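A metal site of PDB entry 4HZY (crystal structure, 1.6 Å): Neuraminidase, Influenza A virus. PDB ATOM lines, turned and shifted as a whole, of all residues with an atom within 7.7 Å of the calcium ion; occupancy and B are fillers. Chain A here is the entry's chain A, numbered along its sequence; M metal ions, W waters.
OD2 of Asp 213 is in hydrogen-bond range of OH of Tyr 235 (2.7 Å).
N of Gly 266 sits close to O of Thr 244, at 3.1 Å.
The guanidinium group (NH2) of Arg 220 lies within salt-bridge range of the side-chain carboxylate (OD1) of Asp 243 (3.4 Å).
O of Gly 266 lies within hydrogen-bond range of NH2 of Arg 212 (3.1 Å).
The backbone carbonyl oxygen (O) of Asp 243 is in hydrogen-bond range of the guanidinium group (NH2) of Arg 246, at 3.0 Å.
The backbone NH (N) of Asp 243 is in hydrogen-bond range of the backbone carbonyl oxygen (O) of Ser 218, 3.2 Å away.
OD1 of Asp 213 sits at hydrogen-bond distance from N of Trp 215 (2.8 Å).
The side-chain carboxylate (OD1) of Asp 213 is in hydrogen-bond range of the backbone NH (N) of Gly 217 (3.0 Å).
Merely in contact with the calcium ion: Gly 266 (3.9 Å).
Five residues have an atom within 4 Å of the calcium ion: Asp 213, Gly 217, Asp 243, Gly 263 and Gly 266.
O of Asp 213 is bound to the calcium ion, at 2.3 Å.
The backbone carbonyl oxygen (O) of Gly 217 is bound to the calcium ion (2.3 Å).
The calcium ion is bound by O of Gly 263 (2.4 Å).
The calcium ion is bound by water W1 (2.4 Å).
The calcium ion is bound by OD2 of Asp 243 (2.4 Å).
Water W1 bridges O of Pro 245 (2.7 Å) and O of Asn 262 (2.8 Å).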
ATOM      1  N   CYS A 211       0.579 -31.959  -6.248  1.00  0.00           N
ATOM      2  CA  CYS A 211      -0.683 -32.177  -5.556  1.00  0.00           C
ATOM      3  C   CYS A 211      -1.688 -31.029  -5.734  1.00  0.00           C
ATOM      4  O   CYS A 211      -1.572 -30.198  -6.645  1.00  0.00           O
ATOM      5  CB  CYS A 211      -0.414 -32.442  -4.061  1.00  0.00           C
ATOM      6  SG  CYS A 211       1.046 -33.508  -3.804  1.00  0.00           S
ATOM      7  N   ARG A 212      -2.685 -31.001  -4.856  1.00  0.00           N
ATOM      8  CA  ARG A 212      -3.786 -30.046  -4.912  1.00  0.00           C
ATOM      9  C   ARG A 212      -3.847 -29.226  -3.622  1.00  0.00           C
ATOM     10  O   ARG A 212      -3.998 -29.778  -2.540  1.00  0.00           O
ATOM     11  CB  ARG A 212      -5.097 -30.819  -5.107  1.00  0.00           C
ATOM     12  CG  ARG A 212      -6.394 -29.996  -4.947  1.00  0.00           C
ATOM     13  CD  ARG A 212      -7.596 -30.937  -5.153  1.00  0.00           C
ATOM     14  NE  ARG A 212      -8.886 -30.297  -4.874  1.00  0.00           N
ATOM     15  CZ  ARG A 212     -10.068 -30.889  -5.017  1.00  0.00           C
ATOM     16  NH1 ARG A 212     -10.133 -32.146  -5.445  1.00  0.00           N
ATOM     17  NH2 ARG A 212     -11.180 -30.236  -4.733  1.00  0.00           N
ATOM     18  N   ASP A 213      -3.734 -27.907  -3.759  1.00  0.00           N
ATOM     19  CA  ASP A 213      -3.954 -26.984  -2.654  1.00  0.00           C
ATOM     20  C   ASP A 213      -5.395 -26.547  -2.828  1.00  0.00           C
ATOM     21  O   ASP A 213      -5.739 -25.991  -3.863  1.00  0.00           O
ATOM     22  CB  ASP A 213      -2.967 -25.806  -2.753  1.00  0.00           C
ATOM     23  CG  ASP A 213      -3.235 -24.709  -1.726  1.00  0.00           C
ATOM     24  OD1 ASP A 213      -4.411 -24.397  -1.483  1.00  0.00           O
ATOM     25  OD2 ASP A 213      -2.264 -24.135  -1.186  1.00  0.00           O
ATOM     26  N   ASN A 214      -6.254 -26.848  -1.864  1.00  0.00           N
ATOM     27  CA  ASN A 214      -7.669 -26.558  -2.023  1.00  0.00           C
ATOM     28  C   ASN A 214      -8.113 -25.320  -1.250  1.00  0.00           C
ATOM     29  O   ASN A 214      -9.301 -25.086  -1.059  1.00  0.00           O
ATOM     30  CB  ASN A 214      -8.538 -27.779  -1.672  1.00  0.00           C
ATOM     31  CG  ASN A 214      -8.464 -28.133  -0.204  1.00  0.00           C
ATOM     32  OD1 ASN A 214      -9.169 -29.030   0.272  1.00  0.00           O
ATOM     33  ND2 ASN A 214      -7.601 -27.451   0.534  1.00  0.00           N
ATOM     34  N   TRP A 215      -7.138 -24.529  -0.807  1.00  0.00           N
ATOM     35  CA  TRP A 215      -7.467 -23.366   0.009  1.00  0.00           C
ATOM     36  C   TRP A 215      -6.948 -22.038  -0.542  1.00  0.00           C
ATOM     37  O   TRP A 215      -7.726 -21.144  -0.869  1.00  0.00           O
ATOM     38  CB  TRP A 215      -7.011 -23.561   1.460  1.00  0.00           C
ATOM     39  CG  TRP A 215      -7.282 -22.370   2.328  1.00  0.00           C
ATOM     40  CD1 TRP A 215      -6.368 -21.458   2.773  1.00  0.00           C
ATOM     41  CD2 TRP A 215      -8.543 -21.965   2.867  1.00  0.00           C
ATOM     42  NE1 TRP A 215      -6.985 -20.515   3.552  1.00  0.00           N
ATOM     43  CE2 TRP A 215      -8.326 -20.797   3.619  1.00  0.00           C
ATOM     44  CE3 TRP A 215      -9.841 -22.475   2.767  1.00  0.00           C
ATOM     45  CZ2 TRP A 215      -9.354 -20.138   4.284  1.00  0.00           C
ATOM     46  CZ3 TRP A 215     -10.859 -21.820   3.433  1.00  0.00           C
ATOM     47  CH2 TRP A 215     -10.612 -20.660   4.180  1.00  0.00           C
ATOM     48  N   LYS A 216      -5.628 -21.898  -0.626  1.00  0.00           N
ATOM     49  CA  LYS A 216      -5.045 -20.614  -1.001  1.00  0.00           C
ATOM     50  C   LYS A 216      -4.241 -20.609  -2.299  1.00  0.00           C
ATOM     51  O   LYS A 216      -3.829 -19.545  -2.767  1.00  0.00           O
ATOM     52  CB  LYS A 216      -4.171 -20.073   0.140  1.00  0.00           C
ATOM     53  CG  LYS A 216      -4.947 -19.746   1.404  1.00  0.00           C
ATOM     54  CD  LYS A 216      -4.836 -18.269   1.747  1.00  0.00           C
ATOM     55  CE  LYS A 216      -5.612 -17.942   3.011  1.00  0.00           C
ATOM     56  NZ  LYS A 216      -6.515 -16.767   2.811  1.00  0.00           N
ATOM     57  N   GLY A 217      -3.998 -21.783  -2.875  1.00  0.00           N
ATOM     58  CA  GLY A 217      -3.102 -21.845  -4.028  1.00  0.00           C
ATOM     59  C   GLY A 217      -3.719 -22.300  -5.340  1.00  0.00           C
ATOM     60  O   GLY A 217      -4.299 -23.371  -5.400  1.00  0.00           O
ATOM     61  N   SER A 218      -3.595 -21.469  -6.365  1.00  0.00           N
ATOM     62  CA  SER A 218      -4.008 -21.838  -7.722  1.00  0.00           C
ATOM     63  C   SER A 218      -2.822 -22.496  -8.422  1.00  0.00           C
ATOM     64  O   SER A 218      -2.981 -23.117  -9.468  1.00  0.00           O
ATOM     65  CB  SER A 218      -4.482 -20.614  -8.522  1.00  0.00           C
ATOM     66  OG  SER A 218      -3.509 -19.576  -8.477  1.00  0.00           O
ATOM     67  N   ASN A 219      -1.633 -22.336  -7.827  1.00  0.00           N
ATOM     68  CA  ASN A 219      -0.431 -23.077  -8.214  1.00  0.00           C
ATOM     69  C   ASN A 219      -0.383 -24.384  -7.412  1.00  0.00           C
ATOM     70  O   ASN A 219      -0.935 -24.460  -6.311  1.00  0.00           O
ATOM     71  CB  ASN A 219       0.841 -22.229  -8.001  1.00  0.00           C
ATOM     72  CG  ASN A 219       0.948 -21.626  -6.592  1.00  0.00           C
ATOM     73  OD1 ASN A 219      -0.039 -21.521  -5.864  1.00  0.00           O
ATOM     74  ND2 ASN A 219       2.155 -21.212  -6.230  1.00  0.00           N
ATOM     75  N   ARG A 220       0.247 -25.424  -7.968  1.00  0.00           N
ATOM     76  CA  ARG A 220       0.247 -26.716  -7.301  1.00  0.00           C
ATOM     77  C   ARG A 220       1.440 -26.930  -6.368  1.00  0.00           C
ATOM     78  O   ARG A 220       2.571 -26.668  -6.735  1.00  0.00           O
ATOM     79  CB  ARG A 220       0.209 -27.847  -8.338  1.00  0.00           C
ATOM     80  CG  ARG A 220      -1.100 -27.912  -9.100  1.00  0.00           C
ATOM     81  CD  ARG A 220      -1.273 -29.271  -9.789  1.00  0.00           C
ATOM     82  NE  ARG A 220      -2.533 -29.315 -10.534  1.00  0.00           N
ATOM     83  CZ  ARG A 220      -3.717 -29.521  -9.967  1.00  0.00           C
ATOM     84  NH1 ARG A 220      -3.794 -29.693  -8.664  1.00  0.00           N
ATOM     85  NH2 ARG A 220      -4.835 -29.537 -10.712  1.00  0.00           N
ATOM     86  N   PRO A 221       1.168 -27.435  -5.158  1.00  0.00           N
ATOM     87  CA  PRO A 221       2.264 -27.794  -4.250  1.00  0.00           C
ATOM     88  C   PRO A 221       2.937 -29.074  -4.722  1.00  0.00           C
ATOM     89  O   PRO A 221       2.317 -29.854  -5.454  1.00  0.00           O
ATOM     90  CB  PRO A 221       1.532 -28.042  -2.926  1.00  0.00           C
ATOM     91  CG  PRO A 221       0.161 -28.481  -3.345  1.00  0.00           C
ATOM     92  CD  PRO A 221      -0.156 -27.687  -4.573  1.00  0.00           C
ATOM     93  N   TYR A 235       6.040 -24.933  -4.192  1.00  0.00           N
ATOM     94  CA  TYR A 235       4.950 -24.832  -5.168  1.00  0.00           C
ATOM     95  C   TYR A 235       5.582 -24.750  -6.554  1.00  0.00           C
ATOM     96  O   TYR A 235       6.702 -24.265  -6.704  1.00  0.00           O
ATOM     97  CB  TYR A 235       4.060 -23.607  -4.910  1.00  0.00           C
ATOM     98  CG  TYR A 235       3.078 -23.795  -3.782  1.00  0.00           C
ATOM     99  CD1 TYR A 235       3.469 -23.654  -2.450  1.00  0.00           C
ATOM    100  CD2 TYR A 235       1.747 -24.098  -4.044  1.00  0.00           C
ATOM    101  CE1 TYR A 235       2.565 -23.825  -1.426  1.00  0.00           C
ATOM    102  CE2 TYR A 235       0.833 -24.273  -3.034  1.00  0.00           C
ATOM    103  CZ  TYR A 235       1.247 -24.135  -1.718  1.00  0.00           C
ATOM    104  OH  TYR A 235       0.348 -24.326  -0.708  1.00  0.00           O
ATOM    105  N   SER A 242      -1.819 -24.221 -12.807  1.00  0.00           N
ATOM    106  CA  SER A 242      -2.422 -25.412 -13.375  1.00  0.00           C
ATOM    107  C   SER A 242      -3.520 -26.056 -12.528  1.00  0.00           C
ATOM    108  O   SER A 242      -3.977 -27.141 -12.856  1.00  0.00           O
ATOM    109  CB  SER A 242      -1.358 -26.445 -13.768  1.00  0.00           C
ATOM    110  OG  SER A 242      -0.642 -26.929 -12.635  1.00  0.00           O
ATOM    111  N   ASP A 243      -3.944 -25.410 -11.441  1.00  0.00           N
ATOM    112  CA  ASP A 243      -5.129 -25.898 -10.749  1.00  0.00           C
ATOM    113  C   ASP A 243      -6.389 -25.324 -11.385  1.00  0.00           C
ATOM    114  O   ASP A 243      -6.322 -24.557 -12.354  1.00  0.00           O
ATOM    115  CB  ASP A 243      -5.085 -25.522  -9.249  1.00  0.00           C
ATOM    116  CG  ASP A 243      -5.828 -26.521  -8.374  1.00  0.00           C
ATOM    117  OD1 ASP A 243      -6.618 -27.342  -8.893  1.00  0.00           O
ATOM    118  OD2 ASP A 243      -5.634 -26.478  -7.145  1.00  0.00           O
ATOM    119  N   THR A 244      -7.544 -25.717 -10.853  1.00  0.00           N
ATOM    120  CA  THR A 244      -8.826 -25.176 -11.291  1.00  0.00           C
ATOM    121  C   THR A 244      -9.685 -24.939 -10.068  1.00  0.00           C
ATOM    122  O   THR A 244      -9.944 -25.861  -9.308  1.00  0.00           O
ATOM    123  CB  THR A 244      -9.575 -26.174 -12.168  1.00  0.00           C
ATOM    124  OG1 THR A 244      -8.716 -26.594 -13.232  1.00  0.00           O
ATOM    125  CG2 THR A 244     -10.822 -25.546 -12.746  1.00  0.00           C
ATOM    126  N   PRO A 245     -10.144 -23.693  -9.867  1.00  0.00           N
ATOM    127  CA  PRO A 245      -9.956 -22.532 -10.749  1.00  0.00           C
ATOM    128  C   PRO A 245      -8.547 -21.985 -10.644  1.00  0.00           C
ATOM    129  O   PRO A 245      -7.767 -22.461  -9.820  1.00  0.00           O
ATOM    130  CB  PRO A 245     -10.954 -21.510 -10.183  1.00  0.00           C
ATOM    131  CG  PRO A 245     -11.044 -21.846  -8.731  1.00  0.00           C
ATOM    132  CD  PRO A 245     -10.952 -23.365  -8.674  1.00  0.00           C
ATOM    133  N   ARG A 246      -8.238 -20.993 -11.471  1.00  0.00           N
ATOM    134  CA  ARG A 246      -6.930 -20.358 -11.466  1.00  0.00           C
ATOM    135  C   ARG A 246      -7.015 -19.023 -12.175  1.00  0.00           C
ATOM    136  O   ARG A 246      -7.959 -18.773 -12.943  1.00  0.00           O
ATOM    137  CB  ARG A 246      -5.901 -21.248 -12.173  1.00  0.00           C
ATOM    138  CG  ARG A 246      -6.248 -21.519 -13.629  1.00  0.00           C
ATOM    139  CD  ARG A 246      -5.163 -22.278 -14.355  1.00  0.00           C
ATOM    140  NE  ARG A 246      -5.516 -22.488 -15.757  1.00  0.00           N
ATOM    141  CZ  ARG A 246      -6.263 -23.501 -16.204  1.00  0.00           C
ATOM    142  NH1 ARG A 246      -6.536 -23.575 -17.492  1.00  0.00           N
ATOM    143  NH2 ARG A 246      -6.722 -24.424 -15.357  1.00  0.00           N
ATOM    144  N   SER A 259      -0.358 -19.078  -4.353  1.00  0.00           N
ATOM    145  CA  SER A 259      -0.563 -17.849  -5.117  1.00  0.00           C
ATOM    146  C   SER A 259      -1.412 -16.840  -4.359  1.00  0.00           C
ATOM    147  O   SER A 259      -1.338 -15.644  -4.628  1.00  0.00           O
ATOM    148  CB  SER A 259      -1.271 -18.175  -6.422  1.00  0.00           C
ATOM    149  OG  SER A 259      -2.586 -18.639  -6.157  1.00  0.00           O
ATOM    150  N   VAL A 261      -4.563 -16.551  -4.622  1.00  0.00           N
ATOM    151  CA  VAL A 261      -5.722 -16.178  -5.436  1.00  0.00           C
ATOM    152  C   VAL A 261      -6.376 -17.428  -6.041  1.00  0.00           C
ATOM    153  O   VAL A 261      -5.671 -18.398  -6.340  1.00  0.00           O
ATOM    154  CB  VAL A 261      -5.337 -15.231  -6.592  1.00  0.00           C
ATOM    155  CG1 VAL A 261      -4.930 -13.863  -6.053  1.00  0.00           C
ATOM    156  CG2 VAL A 261      -4.237 -15.836  -7.438  1.00  0.00           C
ATOM    157  N   ASN A 262      -7.697 -17.398  -6.214  1.00  0.00           N
ATOM    158  CA  ASN A 262      -8.428 -18.530  -6.790  1.00  0.00           C
ATOM    159  C   ASN A 262      -8.034 -19.860  -6.161  1.00  0.00           C
ATOM    160  O   ASN A 262      -7.847 -20.866  -6.861  1.00  0.00           O
ATOM    161  CB  ASN A 262      -8.200 -18.610  -8.303  1.00  0.00           C
ATOM    162  CG  ASN A 262      -8.608 -17.349  -9.014  1.00  0.00           C
ATOM    163  OD1 ASN A 262      -9.802 -17.019  -9.088  1.00  0.00           O
ATOM    164  ND2 ASN A 262      -7.637 -16.626  -9.548  1.00  0.00           N
ATOM    165  N   GLY A 263      -7.954 -19.873  -4.836  1.00  0.00           N
ATOM    166  CA  GLY A 263      -7.415 -21.024  -4.130  1.00  0.00           C
ATOM    167  C   GLY A 263      -8.243 -22.294  -4.160  1.00  0.00           C
ATOM    168  O   GLY A 263      -7.690 -23.386  -4.219  1.00  0.00           O
ATOM    169  N   GLY A 264      -9.557 -22.177  -4.091  1.00  0.00           N
ATOM    170  CA  GLY A 264     -10.402 -23.365  -4.011  1.00  0.00           C
ATOM    171  C   GLY A 264     -11.502 -23.394  -5.050  1.00  0.00           C
ATOM    172  O   GLY A 264     -11.824 -22.365  -5.646  1.00  0.00           O
ATOM    173  N   PRO A 265     -12.101 -24.568  -5.255  1.00  0.00           N
ATOM    174  CA  PRO A 265     -11.803 -25.790  -4.509  1.00  0.00           C
ATOM    175  C   PRO A 265     -10.601 -26.586  -5.036  1.00  0.00           C
ATOM    176  O   PRO A 265     -10.144 -27.490  -4.357  1.00  0.00           O
ATOM    177  CB  PRO A 265     -13.079 -26.628  -4.679  1.00  0.00           C
ATOM    178  CG  PRO A 265     -13.603 -26.204  -6.010  1.00  0.00           C
ATOM    179  CD  PRO A 265     -13.282 -24.733  -6.124  1.00  0.00           C
ATOM    180  N   GLY A 266     -10.106 -26.252  -6.230  1.00  0.00           N
ATOM    181  CA  GLY A 266      -9.059 -27.040  -6.856  1.00  0.00           C
ATOM    182  C   GLY A 266      -9.577 -28.335  -7.469  1.00  0.00           C
ATOM    183  O   GLY A 266     -10.753 -28.675  -7.363  1.00  0.00           O
ATOM    184  N   VAL A 267      -8.672 -29.046  -8.113  1.00  0.00           N
ATOM    185  CA  VAL A 267      -8.965 -30.345  -8.713  1.00  0.00           C
ATOM    186  C   VAL A 267      -7.685 -31.182  -8.670  1.00  0.00           C
ATOM    187  O   VAL A 267      -6.594 -30.640  -8.762  1.00  0.00           O
ATOM    188  CB  VAL A 267      -9.480 -30.199 -10.190  1.00  0.00           C
ATOM    189  CG1 VAL A 267      -8.384 -29.703 -11.124  1.00  0.00           C
ATOM    190  CG2 VAL A 267     -10.054 -31.516 -10.706  1.00  0.00           C
HETATM  191 CA    CA M   1      -6.237 -24.640  -5.642  1.00  0.00          CA
HETATM  192  O   HOH W   1      -7.517 -23.564  -7.361  1.00  0.00           O
